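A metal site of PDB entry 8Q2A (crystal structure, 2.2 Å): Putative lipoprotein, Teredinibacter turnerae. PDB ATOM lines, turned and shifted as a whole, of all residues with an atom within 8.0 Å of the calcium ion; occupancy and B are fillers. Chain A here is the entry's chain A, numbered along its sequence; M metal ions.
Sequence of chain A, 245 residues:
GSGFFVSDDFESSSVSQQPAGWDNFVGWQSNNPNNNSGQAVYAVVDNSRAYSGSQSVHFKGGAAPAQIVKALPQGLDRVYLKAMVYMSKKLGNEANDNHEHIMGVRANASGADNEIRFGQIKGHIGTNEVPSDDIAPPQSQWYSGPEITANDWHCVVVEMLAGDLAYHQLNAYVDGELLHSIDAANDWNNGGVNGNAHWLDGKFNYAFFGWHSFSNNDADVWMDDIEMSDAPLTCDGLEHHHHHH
The calcium ion is bound by the backbone carbonyl oxygen (O) of Gln 55 (2.2 Å), the backbone carbonyl oxygen (O) of Ser 52 (2.3 Å), the side-chain carboxylate (OE2) of Glu 11 (2.3 Å), the side-chain carboxylate (OD1) of Asp 224 (2.4 Å), the side-chain hydroxyl (OG) of Ser 52 (2.4 Å), the backbone carbonyl oxygen (O) of Asp 9 (2.4 Å) and the side-chain carboxylate (OD2) of Asp 224 (2.4 Å). The calcium ion has seven donor atoms within binding distance.
OE1 of Glu 11 sits at hydrogen-bond distance from N of Ser 54, at 2.9 Å. The side-chain amide nitrogen (NE2) of Gln 55 lies within hydrogen-bond range of the backbone carbonyl oxygen (O) of Phe 10 (2.8 Å). The backbone NH of Tyr 51 sits close to the side-chain carboxylate of Asp 224, 3.0 Å away. The side-chain hydroxyl (OG) of Ser 52 lies close to the side-chain carboxylate (OD1) of Asp 225 (2.5 Å).
The nearest printed residue that does not touch the calcium ion is Asp 225 (4.2 Å).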
ATOM      1  N   ASP A   8      -1.363  -5.843 -21.652  1.00  0.00           N
ATOM      2  CA  ASP A   8      -2.458  -5.483 -20.767  1.00  0.00           C
ATOM      3  C   ASP A   8      -2.755  -4.014 -21.032  1.00  0.00           C
ATOM      4  O   ASP A   8      -1.874  -3.159 -20.897  1.00  0.00           O
ATOM      5  CB  ASP A   8      -2.170  -5.785 -19.293  1.00  0.00           C
ATOM      6  CG  ASP A   8      -3.422  -5.934 -18.388  1.00  0.00           C
ATOM      7  OD1 ASP A   8      -4.575  -5.393 -18.755  1.00  0.00           O
ATOM      8  OD2 ASP A   8      -3.259  -6.456 -17.272  1.00  0.00           O
ATOM      9  N   ASP A   9      -4.003  -3.760 -21.460  1.00  0.00           N
ATOM     10  CA  ASP A   9      -4.508  -2.431 -21.677  1.00  0.00           C
ATOM     11  C   ASP A   9      -5.272  -1.938 -20.464  1.00  0.00           C
ATOM     12  O   ASP A   9      -5.752  -0.814 -20.505  1.00  0.00           O
ATOM     13  CB  ASP A   9      -5.352  -2.381 -22.957  1.00  0.00           C
ATOM     14  CG  ASP A   9      -6.636  -3.206 -23.007  1.00  0.00           C
ATOM     15  OD1 ASP A   9      -7.054  -3.745 -21.948  1.00  0.00           O
ATOM     16  OD2 ASP A   9      -7.266  -3.236 -24.124  1.00  0.00           O
ATOM     17  N   PHE A  10      -5.435  -2.786 -19.440  1.00  0.00           N
ATOM     18  CA  PHE A  10      -6.112  -2.441 -18.170  1.00  0.00           C
ATOM     19  C   PHE A  10      -7.614  -2.148 -18.313  1.00  0.00           C
ATOM     20  O   PHE A  10      -8.257  -1.749 -17.346  1.00  0.00           O
ATOM     21  CB  PHE A  10      -5.373  -1.343 -17.400  1.00  0.00           C
ATOM     22  CG  PHE A  10      -3.968  -1.786 -17.081  1.00  0.00           C
ATOM     23  CD1 PHE A  10      -3.746  -2.756 -16.138  1.00  0.00           C
ATOM     24  CD2 PHE A  10      -2.901  -1.323 -17.834  1.00  0.00           C
ATOM     25  CE1 PHE A  10      -2.483  -3.254 -15.923  1.00  0.00           C
ATOM     26  CE2 PHE A  10      -1.611  -1.816 -17.627  1.00  0.00           C
ATOM     27  CZ  PHE A  10      -1.408  -2.798 -16.676  1.00  0.00           C
ATOM     28  N   GLU A  11      -8.219  -2.495 -19.466  1.00  0.00           N
ATOM     29  CA  GLU A  11      -9.606  -2.214 -19.797  1.00  0.00           C
ATOM     30  C   GLU A  11     -10.593  -3.155 -19.087  1.00  0.00           C
ATOM     31  O   GLU A  11     -11.706  -2.731 -18.749  1.00  0.00           O
ATOM     32  CB  GLU A  11      -9.791  -2.188 -21.314  1.00  0.00           C
ATOM     33  CG  GLU A  11      -9.040  -1.030 -21.993  1.00  0.00           C
ATOM     34  CD  GLU A  11      -9.202   0.297 -21.270  1.00  0.00           C
ATOM     35  OE1 GLU A  11     -10.403   0.723 -21.041  1.00  0.00           O
ATOM     36  OE2 GLU A  11      -8.163   0.904 -20.865  1.00  0.00           O
ATOM     37  N   SER A  12     -10.143  -4.387 -18.792  1.00  0.00           N
ATOM     38  CA  SER A  12     -10.955  -5.442 -18.197  1.00  0.00           C
ATOM     39  C   SER A  12     -11.024  -5.272 -16.664  1.00  0.00           C
ATOM     40  O   SER A  12     -12.008  -5.665 -16.038  1.00  0.00           O
ATOM     41  CB  SER A  12     -10.460  -6.820 -18.676  1.00  0.00           C
ATOM     42  OG  SER A  12      -9.346  -7.356 -17.907  1.00  0.00           O
ATOM     43  N   ASP A  46      -7.075   2.935 -12.529  1.00  0.00           N
ATOM     44  CA  ASP A  46      -7.611   4.270 -12.458  1.00  0.00           C
ATOM     45  C   ASP A  46      -8.310   4.541 -13.774  1.00  0.00           C
ATOM     46  O   ASP A  46      -7.804   4.141 -14.818  1.00  0.00           O
ATOM     47  CB  ASP A  46      -6.452   5.267 -12.254  1.00  0.00           C
ATOM     48  CG  ASP A  46      -6.854   6.729 -11.986  1.00  0.00           C
ATOM     49  OD1 ASP A  46      -8.064   6.963 -11.527  1.00  0.00           O
ATOM     50  OD2 ASP A  46      -6.034   7.674 -12.307  1.00  0.00           O
ATOM     51  N   ARG A  49      -7.199   8.875 -15.895  1.00  0.00           N
ATOM     52  CA  ARG A  49      -6.268   9.096 -16.971  1.00  0.00           C
ATOM     53  C   ARG A  49      -6.058   7.770 -17.711  1.00  0.00           C
ATOM     54  O   ARG A  49      -6.065   6.714 -17.055  1.00  0.00           O
ATOM     55  CB  ARG A  49      -5.036   9.695 -16.301  1.00  0.00           C
ATOM     56  CG  ARG A  49      -4.049  10.401 -17.207  1.00  0.00           C
ATOM     57  CD  ARG A  49      -2.691  10.568 -16.492  1.00  0.00           C
ATOM     58  NE  ARG A  49      -2.689  11.495 -15.374  1.00  0.00           N
ATOM     59  CZ  ARG A  49      -2.888  12.811 -15.476  1.00  0.00           C
ATOM     60  NH1 ARG A  49      -3.219  13.338 -16.653  1.00  0.00           N
ATOM     61  NH2 ARG A  49      -2.733  13.583 -14.406  1.00  0.00           N
ATOM     62  N   ALA A  50      -5.932   7.828 -19.053  1.00  0.00           N
ATOM     63  CA  ALA A  50      -5.582   6.645 -19.800  1.00  0.00           C
ATOM     64  C   ALA A  50      -5.010   7.008 -21.152  1.00  0.00           C
ATOM     65  O   ALA A  50      -5.412   7.982 -21.713  1.00  0.00           O
ATOM     66  CB  ALA A  50      -6.776   5.737 -20.014  1.00  0.00           C
ATOM     67  N   TYR A  51      -4.243   6.069 -21.715  1.00  0.00           N
ATOM     68  CA  TYR A  51      -3.782   6.196 -23.070  1.00  0.00           C
ATOM     69  C   TYR A  51      -4.721   5.415 -23.992  1.00  0.00           C
ATOM     70  O   TYR A  51      -5.136   5.933 -25.015  1.00  0.00           O
ATOM     71  CB  TYR A  51      -2.347   5.703 -23.158  1.00  0.00           C
ATOM     72  CG  TYR A  51      -1.817   6.064 -24.535  1.00  0.00           C
ATOM     73  CD1 TYR A  51      -1.372   7.353 -24.796  1.00  0.00           C
ATOM     74  CD2 TYR A  51      -1.826   5.146 -25.574  1.00  0.00           C
ATOM     75  CE1 TYR A  51      -0.970   7.756 -26.053  1.00  0.00           C
ATOM     76  CE2 TYR A  51      -1.407   5.520 -26.836  1.00  0.00           C
ATOM     77  CZ  TYR A  51      -0.957   6.813 -27.075  1.00  0.00           C
ATOM     78  OH  TYR A  51      -0.546   7.155 -28.311  1.00  0.00           O
ATOM     79  N   SER A  52      -5.003   4.174 -23.623  1.00  0.00           N
ATOM     80  CA  SER A  52      -5.921   3.341 -24.388  1.00  0.00           C
ATOM     81  C   SER A  52      -7.212   3.245 -23.589  1.00  0.00           C
ATOM     82  O   SER A  52      -7.165   2.927 -22.415  1.00  0.00           O
ATOM     83  CB  SER A  52      -5.362   1.920 -24.633  1.00  0.00           C
ATOM     84  OG  SER A  52      -5.321   1.173 -23.397  1.00  0.00           O
ATOM     85  N   GLY A  53      -8.355   3.442 -24.222  1.00  0.00           N
ATOM     86  CA  GLY A  53      -9.619   3.123 -23.577  1.00  0.00           C
ATOM     87  C   GLY A  53      -9.878   4.101 -22.451  1.00  0.00           C
ATOM     88  O   GLY A  53      -9.502   5.241 -22.595  1.00  0.00           O
ATOM     89  N   SER A  54     -10.397   3.597 -21.310  1.00  0.00           N
ATOM     90  CA  SER A  54     -10.714   4.423 -20.154  1.00  0.00           C
ATOM     91  C   SER A  54      -9.825   4.125 -18.953  1.00  0.00           C
ATOM     92  O   SER A  54      -9.849   4.895 -17.999  1.00  0.00           O
ATOM     93  CB  SER A  54     -12.185   4.247 -19.773  1.00  0.00           C
ATOM     94  OG  SER A  54     -13.021   4.449 -20.902  1.00  0.00           O
ATOM     95  N   GLN A  55      -9.028   3.069 -18.967  1.00  0.00           N
ATOM     96  CA  GLN A  55      -8.293   2.680 -17.759  1.00  0.00           C
ATOM     97  C   GLN A  55      -6.786   2.528 -17.957  1.00  0.00           C
ATOM     98  O   GLN A  55      -6.297   2.107 -19.016  1.00  0.00           O
ATOM     99  CB  GLN A  55      -8.883   1.398 -17.153  1.00  0.00           C
ATOM    100  CG  GLN A  55     -10.305   1.666 -16.692  1.00  0.00           C
ATOM    101  CD  GLN A  55     -11.051   0.525 -16.069  1.00  0.00           C
ATOM    102  OE1 GLN A  55     -12.120   0.746 -15.514  1.00  0.00           O
ATOM    103  NE2 GLN A  55     -10.466  -0.641 -16.039  1.00  0.00           N
ATOM    104  N   SER A  56      -6.078   2.901 -16.914  1.00  0.00           N
ATOM    105  CA  SER A  56      -4.658   2.778 -16.818  1.00  0.00           C
ATOM    106  C   SER A  56      -4.376   2.213 -15.436  1.00  0.00           C
ATOM    107  O   SER A  56      -5.312   2.092 -14.641  1.00  0.00           O
ATOM    108  CB  SER A  56      -4.003   4.114 -17.066  1.00  0.00           C
ATOM    109  OG  SER A  56      -4.285   5.116 -16.050  1.00  0.00           O
ATOM    110  N   VAL A  57      -3.082   1.976 -15.116  1.00  0.00           N
ATOM    111  CA  VAL A  57      -2.721   1.740 -13.732  1.00  0.00           C
ATOM    112  C   VAL A  57      -2.045   2.987 -13.200  1.00  0.00           C
ATOM    113  O   VAL A  57      -1.234   3.623 -13.839  1.00  0.00           O
ATOM    114  CB  VAL A  57      -1.955   0.431 -13.544  1.00  0.00           C
ATOM    115  CG1 VAL A  57      -0.809   0.345 -14.510  1.00  0.00           C
ATOM    116  CG2 VAL A  57      -1.436   0.253 -12.135  1.00  0.00           C
ATOM    117  N   TRP A 153       2.358  11.671 -22.268  1.00  0.00           N
ATOM    118  CA  TRP A 153       2.439  10.242 -22.505  1.00  0.00           C
ATOM    119  C   TRP A 153       3.659   9.945 -23.363  1.00  0.00           C
ATOM    120  O   TRP A 153       3.741  10.469 -24.430  1.00  0.00           O
ATOM    121  CB  TRP A 153       1.192   9.709 -23.181  1.00  0.00           C
ATOM    122  CG  TRP A 153       0.066   9.586 -22.225  1.00  0.00           C
ATOM    123  CD1 TRP A 153      -1.004  10.408 -22.139  1.00  0.00           C
ATOM    124  CD2 TRP A 153      -0.156   8.522 -21.291  1.00  0.00           C
ATOM    125  NE1 TRP A 153      -1.856   9.958 -21.164  1.00  0.00           N
ATOM    126  CE2 TRP A 153      -1.377   8.806 -20.642  1.00  0.00           C
ATOM    127  CE3 TRP A 153       0.524   7.356 -20.954  1.00  0.00           C
ATOM    128  CZ2 TRP A 153      -1.902   7.981 -19.649  1.00  0.00           C
ATOM    129  CZ3 TRP A 153       0.003   6.555 -19.966  1.00  0.00           C
ATOM    130  CH2 TRP A 153      -1.177   6.861 -19.317  1.00  0.00           C
ATOM    131  N   MET A 223       0.523   4.211 -16.090  1.00  0.00           N
ATOM    132  CA  MET A 223       1.040   3.409 -17.185  1.00  0.00           C
ATOM    133  C   MET A 223      -0.128   2.729 -17.867  1.00  0.00           C
ATOM    134  O   MET A 223      -1.155   2.502 -17.256  1.00  0.00           O
ATOM    135  CB  MET A 223       2.054   2.366 -16.706  1.00  0.00           C
ATOM    136  CG  MET A 223       3.335   2.941 -16.270  1.00  0.00           C
ATOM    137  SD  MET A 223       4.572   1.693 -16.147  1.00  0.00           S
ATOM    138  CE  MET A 223       5.800   2.613 -15.229  1.00  0.00           C
ATOM    139  N   ASP A 224       0.041   2.444 -19.156  1.00  0.00           N
ATOM    140  CA  ASP A 224      -0.991   1.772 -19.889  1.00  0.00           C
ATOM    141  C   ASP A 224      -0.323   1.028 -21.009  1.00  0.00           C
ATOM    142  O   ASP A 224       0.811   1.314 -21.264  1.00  0.00           O
ATOM    143  CB  ASP A 224      -2.028   2.815 -20.353  1.00  0.00           C
ATOM    144  CG  ASP A 224      -3.391   2.306 -20.741  1.00  0.00           C
ATOM    145  OD1 ASP A 224      -3.643   1.127 -20.744  1.00  0.00           O
ATOM    146  OD2 ASP A 224      -4.170   3.149 -21.085  1.00  0.00           O
ATOM    147  N   ASP A 225      -1.061   0.088 -21.626  1.00  0.00           N
ATOM    148  CA  ASP A 225      -0.624  -0.677 -22.776  1.00  0.00           C
ATOM    149  C   ASP A 225       0.743  -1.283 -22.501  1.00  0.00           C
ATOM    150  O   ASP A 225       1.752  -1.026 -23.215  1.00  0.00           O
ATOM    151  CB  ASP A 225      -0.626   0.208 -24.007  1.00  0.00           C
ATOM    152  CG  ASP A 225      -2.007   0.660 -24.469  1.00  0.00           C
ATOM    153  OD1 ASP A 225      -3.064   0.192 -23.882  1.00  0.00           O
ATOM    154  OD2 ASP A 225      -2.044   1.416 -25.454  1.00  0.00           O
ATOM    155  N   ILE A 226       0.808  -1.988 -21.391  1.00  0.00           N
ATOM    156  CA  ILE A 226       2.067  -2.530 -20.980  1.00  0.00           C
ATOM    157  C   ILE A 226       2.255  -3.795 -21.748  1.00  0.00           C
ATOM    158  O   ILE A 226       1.276  -4.518 -21.842  1.00  0.00           O
ATOM    159  CB  ILE A 226       2.108  -2.802 -19.466  1.00  0.00           C
ATOM    160  CG1 ILE A 226       2.229  -1.512 -18.679  1.00  0.00           C
ATOM    161  CG2 ILE A 226       3.199  -3.815 -19.124  1.00  0.00           C
ATOM    162  CD1 ILE A 226       2.284  -1.773 -17.208  1.00  0.00           C
HETATM  163 CA    CA M   1      -5.969   1.497 -21.112  1.00  0.00          CA
